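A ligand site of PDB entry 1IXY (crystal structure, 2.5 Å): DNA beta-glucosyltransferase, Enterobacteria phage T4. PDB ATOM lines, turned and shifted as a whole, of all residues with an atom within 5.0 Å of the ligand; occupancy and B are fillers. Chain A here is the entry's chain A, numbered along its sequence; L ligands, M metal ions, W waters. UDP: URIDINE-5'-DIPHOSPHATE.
The guanidinium group (NH1) of Arg 191 is in salt-bridge range of an oxygen (O2A) of the ligand (2.8 Å).
The backbone carbonyl oxygen (O) of Ile 238 is in hydrogen-bond range of a nitrogen (N3) of the ligand, at 2.9 Å.
An oxygen (O2B) of the ligand is in salt-bridge range of the guanidinium group (NH2) of Arg 195 (2.7 Å).
O4 of the ligand sits at hydrogen-bond distance from N of Ile 238 (2.9 Å).
N of Ser 189 is in hydrogen-bond range of O1A of the ligand (2.9 Å).
O3' of the ligand lies within hydrogen-bond range of OE1 of Glu 272, 2.6 Å away.
NE of Arg 269 is in salt-bridge range of O3B of the ligand (3.1 Å).
The backbone NH (N) of Lys 237 sits at hydrogen-bond distance from the backbone carbonyl oxygen (O) of Gly 214 (3.3 Å).
The backbone NH of Gly 188 sits at hydrogen-bond distance from the backbone carbonyl oxygen of Phe 213.
N of Arg 191 sits close to OG of Ser 189 (3.4 Å).
The side-chain carboxylate (OE2) of Glu 272 is in salt-bridge range of the side-chain amino group (NZ) of Lys 166 (2.7 Å).
NH2 of Arg 191 is in hydrogen-bond range of OH of Tyr 261, 3.4 Å away.
NH1 of Arg 269 is in hydrogen-bond range of O of Gly 187 (2.5 Å).
The guanidinium group of Arg 269 is in hydrogen-bond range of the side-chain hydroxyl of Tyr 186, at 3.2 Å.
N of Phe 213 lies within hydrogen-bond range of O of Tyr 186 (3.0 Å).
Val 18 touches the ligand (CG2 to O2, 3.2 Å).
C of Gly 187 touches C5 of the ligand, at 3.98 Å.
CA of Gly 188 touches O1A of the ligand, at 3.2 Å.
Phe 213 touches the ligand (CD2 to O4, 3.6 Å).
CA of Gly 214 touches O4 of the ligand, 3.4 Å away.
CA of Lys 237 touches O4 of the ligand, 3.3 Å away.
Met 240 touches the ligand (CA to O2, 3.1 Å).
Val 243 touches the ligand.
Tyr 261 touches the ligand.
CD2 of Leu 268 touches O2' of the ligand, 3.9 Å away.
Hydrophobic or aromatic side chains that line the ligand: Val 18, Phe 213, Ile 238, Met 240, Val 243, Tyr 261 and Leu 268.
Within 4 Å of the ligand: Val 18, Gly 187, Gly 188, Ser 189, Arg 191, Arg 195, Phe 213, Gly 214, Lys 237, Ile 238, Met 240, Val 243, Tyr 261, Leu 268, Arg 269 and Glu 272.
The nearest printed residue that does not touch the ligand is Ile 256 (4.02 Å).
Water W2 lies within hydrogen-bond range of O2A of the ligand (2.7 Å) and OG of Ser 189 (3.2 Å).
Water W1 lies within hydrogen-bond range of OH of Tyr 261 (2.7 Å) and O2B of the ligand (3.2 Å).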
ATOM      1  N   VAL A  18     -34.325 -27.489   0.878  1.00  0.00           N
ATOM      2  CA  VAL A  18     -33.463 -27.126   2.006  1.00  0.00           C
ATOM      3  C   VAL A  18     -34.143 -27.384   3.349  1.00  0.00           C
ATOM      4  O   VAL A  18     -33.591 -28.068   4.211  1.00  0.00           O
ATOM      5  CB  VAL A  18     -33.050 -25.652   1.907  1.00  0.00           C
ATOM      6  CG1 VAL A  18     -32.510 -25.167   3.242  1.00  0.00           C
ATOM      7  CG2 VAL A  18     -32.007 -25.502   0.802  1.00  0.00           C
ATOM      8  N   LYS A 166     -23.705 -29.073  11.093  1.00  0.00           N
ATOM      9  CA  LYS A 166     -23.072 -29.691   9.937  1.00  0.00           C
ATOM     10  C   LYS A 166     -21.649 -30.138  10.232  1.00  0.00           C
ATOM     11  O   LYS A 166     -21.262 -31.268   9.916  1.00  0.00           O
ATOM     12  CB  LYS A 166     -23.089 -28.718   8.755  1.00  0.00           C
ATOM     13  CG  LYS A 166     -23.145 -29.403   7.411  1.00  0.00           C
ATOM     14  CD  LYS A 166     -23.744 -28.467   6.359  1.00  0.00           C
ATOM     15  CE  LYS A 166     -24.095 -29.207   5.070  1.00  0.00           C
ATOM     16  NZ  LYS A 166     -24.718 -28.292   4.067  1.00  0.00           N
ATOM     17  N   TYR A 186     -21.558 -18.194  -4.683  1.00  0.00           N
ATOM     18  CA  TYR A 186     -22.497 -17.942  -3.604  1.00  0.00           C
ATOM     19  C   TYR A 186     -23.781 -18.764  -3.785  1.00  0.00           C
ATOM     20  O   TYR A 186     -24.352 -18.815  -4.877  1.00  0.00           O
ATOM     21  CB  TYR A 186     -22.851 -16.452  -3.559  1.00  0.00           C
ATOM     22  CG  TYR A 186     -23.882 -16.087  -2.519  1.00  0.00           C
ATOM     23  CD1 TYR A 186     -25.249 -16.211  -2.782  1.00  0.00           C
ATOM     24  CD2 TYR A 186     -23.499 -15.631  -1.258  1.00  0.00           C
ATOM     25  CE1 TYR A 186     -26.204 -15.883  -1.812  1.00  0.00           C
ATOM     26  CE2 TYR A 186     -24.449 -15.309  -0.283  1.00  0.00           C
ATOM     27  CZ  TYR A 186     -25.792 -15.430  -0.563  1.00  0.00           C
ATOM     28  OH  TYR A 186     -26.711 -15.089   0.404  1.00  0.00           O
ATOM     29  N   GLY A 187     -24.231 -19.414  -2.719  1.00  0.00           N
ATOM     30  CA  GLY A 187     -25.433 -20.205  -2.824  1.00  0.00           C
ATOM     31  C   GLY A 187     -26.518 -19.664  -1.928  1.00  0.00           C
ATOM     32  O   GLY A 187     -26.236 -19.212  -0.813  1.00  0.00           O
ATOM     33  N   GLY A 188     -27.763 -19.725  -2.385  1.00  0.00           N
ATOM     34  CA  GLY A 188     -28.858 -19.228  -1.573  1.00  0.00           C
ATOM     35  C   GLY A 188     -30.063 -18.812  -2.390  1.00  0.00           C
ATOM     36  O   GLY A 188     -30.129 -19.024  -3.606  1.00  0.00           O
ATOM     37  N   SER A 189     -31.025 -18.224  -1.706  1.00  0.00           N
ATOM     38  CA  SER A 189     -32.249 -17.763  -2.346  1.00  0.00           C
ATOM     39  C   SER A 189     -32.243 -16.244  -2.357  1.00  0.00           C
ATOM     40  O   SER A 189     -31.332 -15.605  -1.830  1.00  0.00           O
ATOM     41  CB  SER A 189     -33.466 -18.268  -1.555  1.00  0.00           C
ATOM     42  OG  SER A 189     -33.530 -17.655  -0.276  1.00  0.00           O
ATOM     43  N   ARG A 191     -34.114 -14.362  -0.733  1.00  0.00           N
ATOM     44  CA  ARG A 191     -34.417 -13.876   0.599  1.00  0.00           C
ATOM     45  C   ARG A 191     -35.179 -12.568   0.558  1.00  0.00           C
ATOM     46  O   ARG A 191     -34.892 -11.630   1.302  1.00  0.00           O
ATOM     47  CB  ARG A 191     -33.128 -13.693   1.405  1.00  0.00           C
ATOM     48  CG  ARG A 191     -32.506 -15.000   1.886  1.00  0.00           C
ATOM     49  CD  ARG A 191     -31.390 -14.722   2.888  1.00  0.00           C
ATOM     50  NE  ARG A 191     -31.909 -14.223   4.158  1.00  0.00           N
ATOM     51  CZ  ARG A 191     -32.604 -14.966   5.015  1.00  0.00           C
ATOM     52  NH1 ARG A 191     -32.855 -16.233   4.745  1.00  0.00           N
ATOM     53  NH2 ARG A 191     -33.060 -14.438   6.142  1.00  0.00           N
ATOM     54  N   ARG A 195     -30.915  -8.699   0.763  1.00  0.00           N
ATOM     55  CA  ARG A 195     -29.480  -8.599   0.509  1.00  0.00           C
ATOM     56  C   ARG A 195     -29.226  -8.169  -0.934  1.00  0.00           C
ATOM     57  O   ARG A 195     -28.113  -8.263  -1.428  1.00  0.00           O
ATOM     58  CB  ARG A 195     -28.783  -9.942   0.723  1.00  0.00           C
ATOM     59  CG  ARG A 195     -28.981 -10.520   2.087  1.00  0.00           C
ATOM     60  CD  ARG A 195     -28.331 -11.882   2.223  1.00  0.00           C
ATOM     61  NE  ARG A 195     -28.713 -12.479   3.497  1.00  0.00           N
ATOM     62  CZ  ARG A 195     -28.320 -13.674   3.927  1.00  0.00           C
ATOM     63  NH1 ARG A 195     -27.520 -14.419   3.179  1.00  0.00           N
ATOM     64  NH2 ARG A 195     -28.742 -14.119   5.105  1.00  0.00           N
ATOM     65  N   PHE A 213     -25.583 -20.062  -7.271  1.00  0.00           N
ATOM     66  CA  PHE A 213     -26.465 -21.216  -7.322  1.00  0.00           C
ATOM     67  C   PHE A 213     -27.543 -21.010  -6.281  1.00  0.00           C
ATOM     68  O   PHE A 213     -27.482 -20.047  -5.513  1.00  0.00           O
ATOM     69  CB  PHE A 213     -25.719 -22.530  -7.106  1.00  0.00           C
ATOM     70  CG  PHE A 213     -25.008 -22.651  -5.792  1.00  0.00           C
ATOM     71  CD1 PHE A 213     -23.792 -22.002  -5.591  1.00  0.00           C
ATOM     72  CD2 PHE A 213     -25.505 -23.477  -4.793  1.00  0.00           C
ATOM     73  CE1 PHE A 213     -23.074 -22.180  -4.390  1.00  0.00           C
ATOM     74  CE2 PHE A 213     -24.810 -23.672  -3.589  1.00  0.00           C
ATOM     75  CZ  PHE A 213     -23.583 -23.015  -3.389  1.00  0.00           C
ATOM     76  N   GLY A 214     -28.536 -21.890  -6.278  1.00  0.00           N
ATOM     77  CA  GLY A 214     -29.639 -21.780  -5.345  1.00  0.00           C
ATOM     78  C   GLY A 214     -30.942 -21.481  -6.074  1.00  0.00           C
ATOM     79  O   GLY A 214     -31.016 -21.636  -7.277  1.00  0.00           O
ATOM     80  N   GLY A 236     -29.278 -23.414 -10.941  1.00  0.00           N
ATOM     81  CA  GLY A 236     -30.288 -23.708  -9.943  1.00  0.00           C
ATOM     82  C   GLY A 236     -29.817 -24.207  -8.593  1.00  0.00           C
ATOM     83  O   GLY A 236     -28.660 -24.042  -8.186  1.00  0.00           O
ATOM     84  N   LYS A 237     -30.720 -24.841  -7.875  1.00  0.00           N
ATOM     85  CA  LYS A 237     -30.424 -25.340  -6.553  1.00  0.00           C
ATOM     86  C   LYS A 237     -29.781 -26.715  -6.607  1.00  0.00           C
ATOM     87  O   LYS A 237     -29.920 -27.445  -7.574  1.00  0.00           O
ATOM     88  CB  LYS A 237     -31.703 -25.407  -5.722  1.00  0.00           C
ATOM     89  CG  LYS A 237     -32.839 -26.167  -6.388  1.00  0.00           C
ATOM     90  CD  LYS A 237     -34.129 -26.029  -5.577  1.00  0.00           C
ATOM     91  CE  LYS A 237     -35.329 -26.604  -6.335  1.00  0.00           C
ATOM     92  NZ  LYS A 237     -36.578 -26.476  -5.554  1.00  0.00           N
ATOM     93  N   ILE A 238     -29.072 -27.046  -5.533  1.00  0.00           N
ATOM     94  CA  ILE A 238     -28.435 -28.346  -5.406  1.00  0.00           C
ATOM     95  C   ILE A 238     -28.743 -28.837  -3.992  1.00  0.00           C
ATOM     96  O   ILE A 238     -29.055 -28.052  -3.104  1.00  0.00           O
ATOM     97  CB  ILE A 238     -26.912 -28.237  -5.612  1.00  0.00           C
ATOM     98  CG1 ILE A 238     -26.310 -27.318  -4.567  1.00  0.00           C
ATOM     99  CG2 ILE A 238     -26.608 -27.717  -7.011  1.00  0.00           C
ATOM    100  CD1 ILE A 238     -24.822 -27.339  -4.606  1.00  0.00           C
ATOM    101  N   PRO A 239     -28.658 -30.150  -3.774  1.00  0.00           N
ATOM    102  CA  PRO A 239     -28.940 -30.707  -2.448  1.00  0.00           C
ATOM    103  C   PRO A 239     -28.092 -30.050  -1.381  1.00  0.00           C
ATOM    104  O   PRO A 239     -26.936 -29.677  -1.633  1.00  0.00           O
ATOM    105  CB  PRO A 239     -28.611 -32.181  -2.622  1.00  0.00           C
ATOM    106  CG  PRO A 239     -28.884 -32.411  -4.071  1.00  0.00           C
ATOM    107  CD  PRO A 239     -28.236 -31.214  -4.687  1.00  0.00           C
ATOM    108  N   MET A 240     -28.641 -29.896  -0.178  1.00  0.00           N
ATOM    109  CA  MET A 240     -27.886 -29.281   0.896  1.00  0.00           C
ATOM    110  C   MET A 240     -26.633 -30.065   1.239  1.00  0.00           C
ATOM    111  O   MET A 240     -25.611 -29.486   1.592  1.00  0.00           O
ATOM    112  CB  MET A 240     -28.730 -29.124   2.163  1.00  0.00           C
ATOM    113  CG  MET A 240     -27.988 -28.408   3.281  1.00  0.00           C
ATOM    114  SD  MET A 240     -28.799 -28.425   4.878  1.00  0.00           S
ATOM    115  CE  MET A 240     -29.567 -26.827   4.898  1.00  0.00           C
ATOM    116  N   VAL A 243     -23.640 -28.644  -0.908  1.00  0.00           N
ATOM    117  CA  VAL A 243     -23.239 -27.241  -0.886  1.00  0.00           C
ATOM    118  C   VAL A 243     -21.736 -27.000  -0.776  1.00  0.00           C
ATOM    119  O   VAL A 243     -21.150 -26.337  -1.634  1.00  0.00           O
ATOM    120  CB  VAL A 243     -23.980 -26.490   0.248  1.00  0.00           C
ATOM    121  CG1 VAL A 243     -23.374 -25.115   0.479  1.00  0.00           C
ATOM    122  CG2 VAL A 243     -25.446 -26.363  -0.110  1.00  0.00           C
ATOM    123  N   ILE A 256     -22.373 -13.145   3.206  1.00  0.00           N
ATOM    124  CA  ILE A 256     -23.198 -11.965   3.426  1.00  0.00           C
ATOM    125  C   ILE A 256     -24.427 -12.386   4.210  1.00  0.00           C
ATOM    126  O   ILE A 256     -24.798 -13.559   4.222  1.00  0.00           O
ATOM    127  CB  ILE A 256     -23.653 -11.312   2.099  1.00  0.00           C
ATOM    128  CG1 ILE A 256     -24.107 -12.377   1.110  1.00  0.00           C
ATOM    129  CG2 ILE A 256     -22.554 -10.437   1.547  1.00  0.00           C
ATOM    130  CD1 ILE A 256     -24.669 -11.822  -0.154  1.00  0.00           C
ATOM    131  N   TYR A 261     -28.105 -10.018  10.938  1.00  0.00           N
ATOM    132  CA  TYR A 261     -27.281 -11.226  10.958  1.00  0.00           C
ATOM    133  C   TYR A 261     -25.879 -10.707  11.265  1.00  0.00           C
ATOM    134  O   TYR A 261     -24.985 -11.456  11.661  1.00  0.00           O
ATOM    135  CB  TYR A 261     -27.257 -11.900   9.586  1.00  0.00           C
ATOM    136  CG  TYR A 261     -28.301 -12.981   9.386  1.00  0.00           C
ATOM    137  CD1 TYR A 261     -29.520 -12.949  10.062  1.00  0.00           C
ATOM    138  CD2 TYR A 261     -28.089 -14.000   8.454  1.00  0.00           C
ATOM    139  CE1 TYR A 261     -30.499 -13.901   9.815  1.00  0.00           C
ATOM    140  CE2 TYR A 261     -29.071 -14.960   8.202  1.00  0.00           C
ATOM    141  CZ  TYR A 261     -30.273 -14.903   8.888  1.00  0.00           C
ATOM    142  OH  TYR A 261     -31.256 -15.828   8.639  1.00  0.00           O
ATOM    143  N   THR A 267     -24.103 -17.943  10.598  1.00  0.00           N
ATOM    144  CA  THR A 267     -24.907 -18.861   9.815  1.00  0.00           C
ATOM    145  C   THR A 267     -24.218 -20.148   9.377  1.00  0.00           C
ATOM    146  O   THR A 267     -22.997 -20.294   9.467  1.00  0.00           O
ATOM    147  CB  THR A 267     -25.466 -18.146   8.575  1.00  0.00           C
ATOM    148  OG1 THR A 267     -24.375 -17.595   7.809  1.00  0.00           O
ATOM    149  CG2 THR A 267     -26.397 -17.028   8.977  1.00  0.00           C
ATOM    150  N   LEU A 268     -25.043 -21.071   8.890  1.00  0.00           N
ATOM    151  CA  LEU A 268     -24.583 -22.359   8.420  1.00  0.00           C
ATOM    152  C   LEU A 268     -23.601 -22.229   7.266  1.00  0.00           C
ATOM    153  O   LEU A 268     -22.581 -22.938   7.225  1.00  0.00           O
ATOM    154  CB  LEU A 268     -25.801 -23.181   7.982  1.00  0.00           C
ATOM    155  CG  LEU A 268     -25.554 -24.565   7.406  1.00  0.00           C
ATOM    156  CD1 LEU A 268     -24.623 -25.331   8.317  1.00  0.00           C
ATOM    157  CD2 LEU A 268     -26.873 -25.302   7.290  1.00  0.00           C
ATOM    158  N   ARG A 269     -23.891 -21.339   6.327  1.00  0.00           N
ATOM    159  CA  ARG A 269     -23.020 -21.162   5.168  1.00  0.00           C
ATOM    160  C   ARG A 269     -21.610 -20.797   5.615  1.00  0.00           C
ATOM    161  O   ARG A 269     -20.637 -21.167   4.955  1.00  0.00           O
ATOM    162  CB  ARG A 269     -23.576 -20.098   4.204  1.00  0.00           C
ATOM    163  CG  ARG A 269     -23.250 -18.664   4.558  1.00  0.00           C
ATOM    164  CD  ARG A 269     -23.494 -17.710   3.392  1.00  0.00           C
ATOM    165  NE  ARG A 269     -24.894 -17.663   2.963  1.00  0.00           N
ATOM    166  CZ  ARG A 269     -25.328 -18.135   1.797  1.00  0.00           C
ATOM    167  NH1 ARG A 269     -24.480 -18.680   0.940  1.00  0.00           N
ATOM    168  NH2 ARG A 269     -26.627 -18.085   1.514  1.00  0.00           N
ATOM    169  N   GLU A 272     -20.188 -23.947   5.988  1.00  0.00           N
ATOM    170  CA  GLU A 272     -20.178 -24.641   4.694  1.00  0.00           C
ATOM    171  C   GLU A 272     -19.098 -24.056   3.805  1.00  0.00           C
ATOM    172  O   GLU A 272     -18.444 -24.767   3.037  1.00  0.00           O
ATOM    173  CB  GLU A 272     -21.520 -24.496   3.977  1.00  0.00           C
ATOM    174  CG  GLU A 272     -22.729 -24.868   4.809  1.00  0.00           C
ATOM    175  CD  GLU A 272     -24.010 -24.741   4.022  1.00  0.00           C
ATOM    176  OE1 GLU A 272     -24.112 -23.800   3.199  1.00  0.00           O
ATOM    177  OE2 GLU A 272     -24.924 -25.560   4.232  1.00  0.00           O
HETATM  178  N1  UDP L   1     -28.560 -24.108   0.139  1.00  0.00           N
HETATM  179  C2  UDP L   1     -28.778 -25.399  -0.351  1.00  0.00           C
HETATM  180  N3  UDP L   1     -28.799 -25.492  -1.722  1.00  0.00           N
HETATM  181  C4  UDP L   1     -28.621 -24.478  -2.618  1.00  0.00           C
HETATM  182  C5  UDP L   1     -28.352 -23.195  -2.032  1.00  0.00           C
HETATM  183  C6  UDP L   1     -28.347 -23.064  -0.709  1.00  0.00           C
HETATM  184  O2  UDP L   1     -28.925 -26.369   0.379  1.00  0.00           O
HETATM  185  O4  UDP L   1     -28.783 -24.703  -3.812  1.00  0.00           O
HETATM  186  C1' UDP L   1     -28.610 -23.926   1.593  1.00  0.00           C
HETATM  187  C2' UDP L   1     -27.235 -23.967   2.284  1.00  0.00           C
HETATM  188  O2' UDP L   1     -27.345 -24.663   3.503  1.00  0.00           O
HETATM  189  C3' UDP L   1     -26.940 -22.470   2.461  1.00  0.00           C
HETATM  190  C4' UDP L   1     -28.321 -21.913   2.770  1.00  0.00           C
HETATM  191  O4' UDP L   1     -29.188 -22.662   1.878  1.00  0.00           O
HETATM  192  O3' UDP L   1     -26.072 -22.209   3.567  1.00  0.00           O
HETATM  193  C5' UDP L   1     -28.462 -20.436   2.565  1.00  0.00           C
HETATM  194  O5' UDP L   1     -29.786 -20.022   2.847  1.00  0.00           O
HETATM  195  PA  UDP L   1     -30.232 -18.523   2.583  1.00  0.00           P
HETATM  196  O1A UDP L   1     -30.228 -18.282   1.123  1.00  0.00           O
HETATM  197  O2A UDP L   1     -31.481 -18.281   3.362  1.00  0.00           O
HETATM  198  O3A UDP L   1     -29.006 -17.650   3.232  1.00  0.00           O
HETATM  199  PB  UDP L   1     -28.552 -17.464   4.794  1.00  0.00           P
HETATM  200  O1B UDP L   1     -28.444 -18.865   5.371  1.00  0.00           O
HETATM  201  O2B UDP L   1     -29.663 -16.637   5.432  1.00  0.00           O
HETATM  202  O3B UDP L   1     -27.217 -16.721   4.752  1.00  0.00           O
HETATM  203 MG    MG M   1     -30.301 -20.541   8.008  1.00  0.00          MG
HETATM  204  O   HOH W   1     -30.263 -18.287   8.082  1.00  0.00           O
HETATM  205  O   HOH W   2     -33.835 -19.275   2.493  1.00  0.00           O
